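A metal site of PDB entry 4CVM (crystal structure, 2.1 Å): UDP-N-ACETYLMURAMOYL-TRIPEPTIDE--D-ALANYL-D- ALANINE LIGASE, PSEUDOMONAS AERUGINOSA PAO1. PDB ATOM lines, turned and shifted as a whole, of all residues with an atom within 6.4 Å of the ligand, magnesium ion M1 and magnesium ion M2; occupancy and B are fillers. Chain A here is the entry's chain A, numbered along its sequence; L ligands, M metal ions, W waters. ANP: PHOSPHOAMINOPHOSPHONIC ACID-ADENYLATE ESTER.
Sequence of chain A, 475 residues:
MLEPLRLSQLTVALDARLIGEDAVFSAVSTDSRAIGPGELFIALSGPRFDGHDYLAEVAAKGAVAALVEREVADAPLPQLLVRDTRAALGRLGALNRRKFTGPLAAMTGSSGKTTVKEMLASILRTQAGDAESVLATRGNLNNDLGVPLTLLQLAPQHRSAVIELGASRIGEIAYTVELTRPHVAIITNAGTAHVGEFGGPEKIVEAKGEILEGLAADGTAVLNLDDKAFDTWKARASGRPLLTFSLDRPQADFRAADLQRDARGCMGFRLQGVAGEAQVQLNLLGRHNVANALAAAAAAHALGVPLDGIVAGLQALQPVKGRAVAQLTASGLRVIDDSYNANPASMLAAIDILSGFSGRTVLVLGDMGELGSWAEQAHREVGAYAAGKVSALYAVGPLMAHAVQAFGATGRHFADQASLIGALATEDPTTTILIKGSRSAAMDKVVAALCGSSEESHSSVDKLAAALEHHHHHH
Merely in contact with the ligand: Ser 110 (3.7 Å), Asn 142 (3.5 Å), Asn 189 (3.5 Å), Thr 192 (3.7 Å), His 288 (3.5 Å) and Ala 349 (3.5 Å).
Hydrophobic or aromatic side chains within 4 Å of the ligand: His 288 and Ala 349.
Within 4 Å of the ligand: Ser 110, Ser 111, Gly 112, Lys 113, Thr 114, Thr 115, Asn 140, Asn 142, Glu 164, Asn 189, Thr 192, His 288, Asn 292 and Ala 349.
Water W1 lies within hydrogen-bond range of a nitrogen (N3B) of the ligand and the backbone carbonyl oxygen (O) of Ser 110.
Water W2 lies within hydrogen-bond range of N6 of the ligand, O of Thr 188 and ND2 of Asn 189.
The side-chain amide oxygen of Asn 189 is in hydrogen-bond range of the side-chain hydroxyl of Thr 188 (3.4 Å).
O of Asn 142 is in hydrogen-bond range of N of Gly 166 (2.8 Å).
OG1 of Thr 192 is in hydrogen-bond range of OG of Ser 111 (2.9 Å).
N of Ser 110 lies within hydrogen-bond range of OD1 of Asn 189, at 3.0 Å.
OD1 of Asn 189 sits at hydrogen-bond distance from N of Ser 111 (2.9 Å).
The side-chain hydroxyl (OG1) of Thr 188 sits at hydrogen-bond distance from the backbone carbonyl oxygen (O) of Ser 111 (2.6 Å).
The backbone carbonyl oxygen (O) of Gly 109 is in hydrogen-bond range of the side-chain amino group (NZ) of Lys 113 (3.0 Å).
The side-chain amide oxygen of Asn 289 lies within hydrogen-bond range of the side-chain amide nitrogen of Asn 292.
The side-chain amide oxygen (OD1) of Asn 140 is bound to magnesium ion M1.
O2B of the ligand is bound to magnesium ion M1, at 2.1 Å.
O2G of the ligand binds magnesium ion M1 (2.1 Å).
OG1 of Thr 114 is bound to magnesium ion M1 (2.3 Å).
The side-chain carboxylate (OE2) of Glu 164 binds magnesium ion M1, 2.4 Å away.
Two residues have an atom within 4 Å of magnesium ion M2: Thr 114 and Asn 140.
The nearest printed residue that does not touch magnesium ion M2 is Glu 164 (4.3 Å).
N3 of the ligand is in hydrogen-bond range of OG of Ser 111, 3.2 Å away.
The backbone NH of Thr 115 lies within hydrogen-bond range of an oxygen (O1A) of the ligand (2.9 Å).
A nitrogen (N6) of the ligand sits at hydrogen-bond distance from the side-chain amide oxygen (OD1) of Asn 292 (2.9 Å).
An oxygen (O1B) of the ligand is in salt-bridge range of the side-chain amino group (NZ) of Lys 113 (2.7 Å).
N of Thr 114 sits close to O2B of the ligand (2.9 Å).
The backbone NH (N) of Gly 112 sits at hydrogen-bond distance from an oxygen (O3A) of the ligand (3.0 Å).
An oxygen (O1A) of the ligand lies within hydrogen-bond range of the side-chain hydroxyl of Thr 115 (2.6 Å).
N of Lys 113 lies within hydrogen-bond range of O1B of the ligand, at 2.9 Å.
Within 4 Å of magnesium ion M1: Thr 114, Asn 140 and Glu 164.
Magnesium ion M2 is bound by an oxygen (O2B) of the ligand.
Slightly farther from magnesium ion M2 lies OD1 of Asn 140 (2.6 Å).
Slightly farther from magnesium ion M2 lies the side-chain hydroxyl (OG1) of Thr 114 (2.7 Å).
Slightly farther from magnesium ion M2 lies an oxygen (O2A) of the ligand (2.8 Å).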
ATOM      1  N   GLY A 109      16.439 -29.568 -28.876  1.00  0.00           N
ATOM      2  CA  GLY A 109      16.966 -28.785 -29.967  1.00  0.00           C
ATOM      3  C   GLY A 109      18.158 -27.983 -29.484  1.00  0.00           C
ATOM      4  O   GLY A 109      18.482 -27.936 -28.297  1.00  0.00           O
ATOM      5  N   SER A 110      18.839 -27.348 -30.408  1.00  0.00           N
ATOM      6  CA  SER A 110      19.964 -26.497 -30.033  1.00  0.00           C
ATOM      7  C   SER A 110      19.428 -25.168 -29.558  1.00  0.00           C
ATOM      8  O   SER A 110      19.965 -24.600 -28.617  1.00  0.00           O
ATOM      9  CB  SER A 110      20.942 -26.291 -31.196  1.00  0.00           C
ATOM     10  OG  SER A 110      21.602 -27.479 -31.512  1.00  0.00           O
ATOM     11  N   SER A 111      18.403 -24.649 -30.241  1.00  0.00           N
ATOM     12  CA  SER A 111      17.831 -23.404 -29.817  1.00  0.00           C
ATOM     13  C   SER A 111      16.321 -23.453 -30.031  1.00  0.00           C
ATOM     14  O   SER A 111      15.817 -24.233 -30.863  1.00  0.00           O
ATOM     15  CB  SER A 111      18.458 -22.242 -30.640  1.00  0.00           C
ATOM     16  OG  SER A 111      18.108 -22.464 -31.995  1.00  0.00           O
ATOM     17  N   GLY A 112      15.609 -22.647 -29.248  1.00  0.00           N
ATOM     18  CA  GLY A 112      14.165 -22.524 -29.346  1.00  0.00           C
ATOM     19  C   GLY A 112      13.379 -23.456 -28.427  1.00  0.00           C
ATOM     20  O   GLY A 112      12.156 -23.412 -28.465  1.00  0.00           O
ATOM     21  N   LYS A 113      14.064 -24.228 -27.589  1.00  0.00           N
ATOM     22  CA  LYS A 113      13.416 -25.151 -26.649  1.00  0.00           C
ATOM     23  C   LYS A 113      12.471 -24.454 -25.699  1.00  0.00           C
ATOM     24  O   LYS A 113      11.285 -24.780 -25.648  1.00  0.00           O
ATOM     25  CB  LYS A 113      14.462 -25.918 -25.826  1.00  0.00           C
ATOM     26  CG  LYS A 113      15.320 -26.883 -26.616  1.00  0.00           C
ATOM     27  CD  LYS A 113      16.229 -27.688 -25.702  1.00  0.00           C
ATOM     28  CE  LYS A 113      17.246 -26.858 -24.895  1.00  0.00           C
ATOM     29  NZ  LYS A 113      18.093 -26.112 -25.888  1.00  0.00           N
ATOM     30  N   THR A 114      12.980 -23.424 -25.007  1.00  0.00           N
ATOM     31  CA  THR A 114      12.190 -22.685 -24.036  1.00  0.00           C
ATOM     32  C   THR A 114      11.033 -21.986 -24.710  1.00  0.00           C
ATOM     33  O   THR A 114       9.909 -21.956 -24.193  1.00  0.00           O
ATOM     34  CB  THR A 114      13.103 -21.770 -23.189  1.00  0.00           C
ATOM     35  OG1 THR A 114      13.874 -22.609 -22.351  1.00  0.00           O
ATOM     36  CG2 THR A 114      12.294 -20.831 -22.220  1.00  0.00           C
ATOM     37  N   THR A 115      11.307 -21.412 -25.869  1.00  0.00           N
ATOM     38  CA  THR A 115      10.260 -20.670 -26.555  1.00  0.00           C
ATOM     39  C   THR A 115       9.142 -21.577 -27.062  1.00  0.00           C
ATOM     40  O   THR A 115       7.966 -21.255 -26.907  1.00  0.00           O
ATOM     41  CB  THR A 115      10.868 -19.843 -27.689  1.00  0.00           C
ATOM     42  OG1 THR A 115      11.901 -19.042 -27.131  1.00  0.00           O
ATOM     43  CG2 THR A 115       9.836 -18.950 -28.376  1.00  0.00           C
ATOM     44  N   VAL A 116       9.502 -22.703 -27.676  1.00  0.00           N
ATOM     45  CA  VAL A 116       8.491 -23.666 -28.104  1.00  0.00           C
ATOM     46  C   VAL A 116       7.696 -24.172 -26.884  1.00  0.00           C
ATOM     47  O   VAL A 116       6.455 -24.283 -26.907  1.00  0.00           O
ATOM     48  CB  VAL A 116       9.109 -24.824 -28.871  1.00  0.00           C
ATOM     49  CG1 VAL A 116       8.103 -25.915 -29.088  1.00  0.00           C
ATOM     50  CG2 VAL A 116       9.604 -24.314 -30.194  1.00  0.00           C
ATOM     51  N   GLY A 139      11.730 -22.223 -15.810  1.00  0.00           N
ATOM     52  CA  GLY A 139      13.000 -21.680 -16.359  1.00  0.00           C
ATOM     53  C   GLY A 139      13.610 -22.613 -17.368  1.00  0.00           C
ATOM     54  O   GLY A 139      12.969 -23.080 -18.371  1.00  0.00           O
ATOM     55  N   ASN A 140      14.849 -22.975 -17.070  1.00  0.00           N
ATOM     56  CA  ASN A 140      15.572 -23.849 -17.895  1.00  0.00           C
ATOM     57  C   ASN A 140      15.973 -25.160 -17.231  1.00  0.00           C
ATOM     58  O   ASN A 140      17.040 -25.719 -17.541  1.00  0.00           O
ATOM     59  CB  ASN A 140      16.780 -23.100 -18.348  1.00  0.00           C
ATOM     60  CG  ASN A 140      17.066 -23.332 -19.770  1.00  0.00           C
ATOM     61  OD1 ASN A 140      16.151 -23.236 -20.614  1.00  0.00           O
ATOM     62  ND2 ASN A 140      18.311 -23.647 -20.057  1.00  0.00           N
ATOM     63  N   ASN A 142      16.285 -28.370 -17.318  1.00  0.00           N
ATOM     64  CA  ASN A 142      16.133 -29.317 -18.421  1.00  0.00           C
ATOM     65  C   ASN A 142      17.182 -30.413 -18.542  1.00  0.00           C
ATOM     66  O   ASN A 142      17.169 -31.154 -19.545  1.00  0.00           O
ATOM     67  CB  ASN A 142      16.023 -28.553 -19.753  1.00  0.00           C
ATOM     68  CG  ASN A 142      17.328 -27.891 -20.186  1.00  0.00           C
ATOM     69  OD1 ASN A 142      18.377 -28.201 -19.682  1.00  0.00           O
ATOM     70  ND2 ASN A 142      17.244 -27.020 -21.164  1.00  0.00           N
ATOM     71  N   GLU A 164      10.674 -29.547 -21.183  1.00  0.00           N
ATOM     72  CA  GLU A 164      11.891 -29.236 -21.926  1.00  0.00           C
ATOM     73  C   GLU A 164      13.021 -30.251 -21.627  1.00  0.00           C
ATOM     74  O   GLU A 164      13.327 -30.550 -20.472  1.00  0.00           O
ATOM     75  CB  GLU A 164      12.292 -27.786 -21.584  1.00  0.00           C
ATOM     76  CG  GLU A 164      13.359 -27.229 -22.438  1.00  0.00           C
ATOM     77  CD  GLU A 164      13.739 -25.781 -22.087  1.00  0.00           C
ATOM     78  OE1 GLU A 164      12.903 -24.938 -21.605  1.00  0.00           O
ATOM     79  OE2 GLU A 164      14.889 -25.491 -22.395  1.00  0.00           O
ATOM     80  N   GLY A 166      17.046 -30.817 -22.335  1.00  0.00           N
ATOM     81  CA  GLY A 166      18.320 -30.286 -22.796  1.00  0.00           C
ATOM     82  C   GLY A 166      19.213 -31.401 -23.274  1.00  0.00           C
ATOM     83  O   GLY A 166      19.193 -32.510 -22.711  1.00  0.00           O
ATOM     84  N   THR A 188      13.545 -28.941 -32.466  1.00  0.00           N
ATOM     85  CA  THR A 188      13.506 -27.640 -33.189  1.00  0.00           C
ATOM     86  C   THR A 188      14.524 -27.549 -34.304  1.00  0.00           C
ATOM     87  O   THR A 188      14.211 -27.108 -35.415  1.00  0.00           O
ATOM     88  CB  THR A 188      13.733 -26.458 -32.236  1.00  0.00           C
ATOM     89  OG1 THR A 188      14.980 -26.649 -31.538  1.00  0.00           O
ATOM     90  CG2 THR A 188      12.537 -26.398 -31.255  1.00  0.00           C
ATOM     91  N   ASN A 189      15.742 -27.974 -33.978  1.00  0.00           N
ATOM     92  CA  ASN A 189      16.913 -27.824 -34.837  1.00  0.00           C
ATOM     93  C   ASN A 189      18.156 -28.455 -34.189  1.00  0.00           C
ATOM     94  O   ASN A 189      18.168 -28.796 -32.990  1.00  0.00           O
ATOM     95  CB  ASN A 189      17.227 -26.345 -35.102  1.00  0.00           C
ATOM     96  CG  ASN A 189      17.282 -25.518 -33.840  1.00  0.00           C
ATOM     97  OD1 ASN A 189      18.008 -25.828 -32.882  1.00  0.00           O
ATOM     98  ND2 ASN A 189      16.498 -24.485 -33.804  1.00  0.00           N
ATOM     99  N   THR A 192      22.504 -24.411 -34.396  1.00  0.00           N
ATOM    100  CA  THR A 192      22.323 -22.948 -34.637  1.00  0.00           C
ATOM    101  C   THR A 192      23.491 -22.062 -34.041  1.00  0.00           C
ATOM    102  O   THR A 192      24.257 -22.504 -33.199  1.00  0.00           O
ATOM    103  CB  THR A 192      20.943 -22.473 -34.102  1.00  0.00           C
ATOM    104  OG1 THR A 192      20.803 -22.960 -32.782  1.00  0.00           O
ATOM    105  CG2 THR A 192      19.787 -23.064 -34.936  1.00  0.00           C
ATOM    106  N   ALA A 193      23.655 -20.824 -34.520  1.00  0.00           N
ATOM    107  CA  ALA A 193      24.801 -19.968 -34.099  1.00  0.00           C
ATOM    108  C   ALA A 193      24.869 -19.619 -32.613  1.00  0.00           C
ATOM    109  O   ALA A 193      23.835 -19.568 -31.907  1.00  0.00           O
ATOM    110  CB  ALA A 193      24.801 -18.676 -34.907  1.00  0.00           C
ATOM    111  N   VAL A 195      25.598 -21.143 -29.991  1.00  0.00           N
ATOM    112  CA  VAL A 195      25.075 -22.056 -28.955  1.00  0.00           C
ATOM    113  C   VAL A 195      26.170 -22.748 -28.119  1.00  0.00           C
ATOM    114  O   VAL A 195      27.251 -23.077 -28.628  1.00  0.00           O
ATOM    115  CB  VAL A 195      24.039 -23.052 -29.546  1.00  0.00           C
ATOM    116  CG1 VAL A 195      23.869 -24.273 -28.643  1.00  0.00           C
ATOM    117  CG2 VAL A 195      22.684 -22.353 -29.681  1.00  0.00           C
ATOM    118  N   HIS A 288      13.132 -16.671 -36.708  1.00  0.00           N
ATOM    119  CA  HIS A 288      13.240 -17.961 -36.019  1.00  0.00           C
ATOM    120  C   HIS A 288      12.007 -18.248 -35.127  1.00  0.00           C
ATOM    121  O   HIS A 288      11.710 -19.403 -34.838  1.00  0.00           O
ATOM    122  CB  HIS A 288      14.524 -18.013 -35.175  1.00  0.00           C
ATOM    123  CG  HIS A 288      14.621 -16.962 -34.113  1.00  0.00           C
ATOM    124  ND1 HIS A 288      15.062 -15.680 -34.372  1.00  0.00           N
ATOM    125  CD2 HIS A 288      14.309 -16.987 -32.795  1.00  0.00           C
ATOM    126  CE1 HIS A 288      15.036 -14.969 -33.259  1.00  0.00           C
ATOM    127  NE2 HIS A 288      14.572 -15.730 -32.290  1.00  0.00           N
ATOM    128  N   ASN A 289      11.309 -17.214 -34.664  1.00  0.00           N
ATOM    129  CA  ASN A 289      10.189 -17.410 -33.769  1.00  0.00           C
ATOM    130  C   ASN A 289       8.932 -17.857 -34.559  1.00  0.00           C
ATOM    131  O   ASN A 289       8.053 -18.502 -33.984  1.00  0.00           O
ATOM    132  CB  ASN A 289       9.937 -16.190 -32.915  1.00  0.00           C
ATOM    133  CG  ASN A 289      10.770 -16.193 -31.664  1.00  0.00           C
ATOM    134  OD1 ASN A 289      11.001 -17.252 -31.069  1.00  0.00           O
ATOM    135  ND2 ASN A 289      11.275 -15.021 -31.263  1.00  0.00           N
ATOM    136  N   ALA A 291       9.291 -20.147 -37.025  1.00  0.00           N
ATOM    137  CA  ALA A 291       9.572 -21.606 -37.010  1.00  0.00           C
ATOM    138  C   ALA A 291       9.166 -22.228 -35.617  1.00  0.00           C
ATOM    139  O   ALA A 291       8.595 -23.290 -35.587  1.00  0.00           O
ATOM    140  CB  ALA A 291      11.029 -21.875 -37.315  1.00  0.00           C
ATOM    141  N   ASN A 292       9.484 -21.546 -34.519  1.00  0.00           N
ATOM    142  CA  ASN A 292       9.090 -21.973 -33.197  1.00  0.00           C
ATOM    143  C   ASN A 292       7.547 -22.076 -33.078  1.00  0.00           C
ATOM    144  O   ASN A 292       7.035 -23.059 -32.551  1.00  0.00           O
ATOM    145  CB  ASN A 292       9.657 -21.089 -32.072  1.00  0.00           C
ATOM    146  CG  ASN A 292      11.182 -21.172 -31.995  1.00  0.00           C
ATOM    147  OD1 ASN A 292      11.775 -22.170 -32.411  1.00  0.00           O
ATOM    148  ND2 ASN A 292      11.789 -20.188 -31.377  1.00  0.00           N
ATOM    149  N   ALA A 324      14.106  -9.135 -24.873  1.00  0.00           N
ATOM    150  CA  ALA A 324      13.701  -8.744 -26.214  1.00  0.00           C
ATOM    151  C   ALA A 324      12.224  -8.320 -26.262  1.00  0.00           C
ATOM    152  O   ALA A 324      11.484  -8.834 -27.067  1.00  0.00           O
ATOM    153  CB  ALA A 324      13.988  -9.863 -27.195  1.00  0.00           C
ATOM    154  N   ALA A 349      23.453 -12.943 -30.036  1.00  0.00           N
ATOM    155  CA  ALA A 349      22.080 -13.191 -30.471  1.00  0.00           C
ATOM    156  C   ALA A 349      21.298 -11.869 -30.601  1.00  0.00           C
ATOM    157  O   ALA A 349      20.497 -11.715 -31.528  1.00  0.00           O
ATOM    158  CB  ALA A 349      21.368 -14.162 -29.539  1.00  0.00           C
ATOM    159  N   ALA A 350      21.535 -10.922 -29.682  1.00  0.00           N
ATOM    160  CA  ALA A 350      20.883  -9.598 -29.718  1.00  0.00           C
ATOM    161  C   ALA A 350      21.241  -8.816 -30.973  1.00  0.00           C
ATOM    162  O   ALA A 350      20.377  -8.347 -31.694  1.00  0.00           O
ATOM    163  CB  ALA A 350      21.257  -8.757 -28.464  1.00  0.00           C
ATOM    164  N   ILE A 353      19.456 -10.091 -34.036  1.00  0.00           N
ATOM    165  CA  ILE A 353      18.089  -9.591 -34.078  1.00  0.00           C
ATOM    166  C   ILE A 353      18.030  -8.147 -34.607  1.00  0.00           C
ATOM    167  O   ILE A 353      17.162  -7.815 -35.433  1.00  0.00           O
ATOM    168  CB  ILE A 353      17.366  -9.683 -32.692  1.00  0.00           C
ATOM    169  CG1 ILE A 353      17.153 -11.148 -32.298  1.00  0.00           C
ATOM    170  CG2 ILE A 353      16.035  -8.952 -32.720  1.00  0.00           C
ATOM    171  CD1 ILE A 353      16.376 -11.328 -30.999  1.00  0.00           C
HETATM  172  PG  ANP L   1      18.994 -23.364 -23.779  1.00  0.00           P
HETATM  173  O1G ANP L   1      19.720 -24.510 -24.454  1.00  0.00           O
HETATM  174  O2G ANP L   1      17.974 -24.022 -22.870  1.00  0.00           O
HETATM  175  O3G ANP L   1      19.724 -22.196 -23.263  1.00  0.00           O
HETATM  176  PB  ANP L   1      16.755 -22.788 -25.706  1.00  0.00           P
HETATM  177  O1B ANP L   1      16.832 -23.884 -26.724  1.00  0.00           O
HETATM  178  O2B ANP L   1      15.800 -22.949 -24.515  1.00  0.00           O
HETATM  179  N3B ANP L   1      18.337 -22.457 -25.101  1.00  0.00           N
HETATM  180  PA  ANP L   1      15.381 -20.242 -26.179  1.00  0.00           P
HETATM  181  O1A ANP L   1      13.975 -20.480 -26.710  1.00  0.00           O
HETATM  182  O2A ANP L   1      15.607 -19.844 -24.706  1.00  0.00           O
HETATM  183  O3A ANP L   1      16.370 -21.464 -26.591  1.00  0.00           O
HETATM  184  O5' ANP L   1      15.929 -19.012 -27.061  1.00  0.00           O
HETATM  185  C5' ANP L   1      17.304 -18.565 -26.882  1.00  0.00           C
HETATM  186  C4' ANP L   1      17.807 -17.809 -28.102  1.00  0.00           C
HETATM  187  O4' ANP L   1      18.074 -18.684 -29.201  1.00  0.00           O
HETATM  188  C3' ANP L   1      16.792 -16.780 -28.635  1.00  0.00           C
HETATM  189  O3' ANP L   1      16.784 -15.514 -27.958  1.00  0.00           O
HETATM  190  C2' ANP L   1      17.233 -16.673 -30.055  1.00  0.00           C
HETATM  191  O2' ANP L   1      18.390 -15.820 -30.129  1.00  0.00           O
HETATM  192  C1' ANP L   1      17.685 -18.079 -30.439  1.00  0.00           C
HETATM  193  N9  ANP L   1      16.623 -18.925 -31.034  1.00  0.00           N
HETATM  194  C8  ANP L   1      15.449 -19.292 -30.427  1.00  0.00           C
HETATM  195  N7  ANP L   1      14.741 -20.123 -31.258  1.00  0.00           N
HETATM  196  C5  ANP L   1      15.502 -20.327 -32.362  1.00  0.00           C
HETATM  197  C6  ANP L   1      15.365 -21.060 -33.630  1.00  0.00           C
HETATM  198  N6  ANP L   1      14.248 -21.794 -33.844  1.00  0.00           N
HETATM  199  N1  ANP L   1      16.368 -20.965 -34.548  1.00  0.00           N
HETATM  200  C2  ANP L   1      17.488 -20.253 -34.333  1.00  0.00           C
HETATM  201  N3  ANP L   1      17.642 -19.531 -33.217  1.00  0.00           N
HETATM  202  C4  ANP L   1      16.730 -19.540 -32.218  1.00  0.00           C
HETATM  203 MG    MG M   1      15.992 -23.396 -22.489  1.00  0.00          MG
HETATM  204 MG    MG M   2      16.277 -21.388 -22.509  1.00  0.00          MG
HETATM  205  O   HOH W   1      20.058 -22.092 -27.289  1.00  0.00           O
HETATM  206  O   HOH W   2      13.939 -24.050 -35.809  1.00  0.00           O
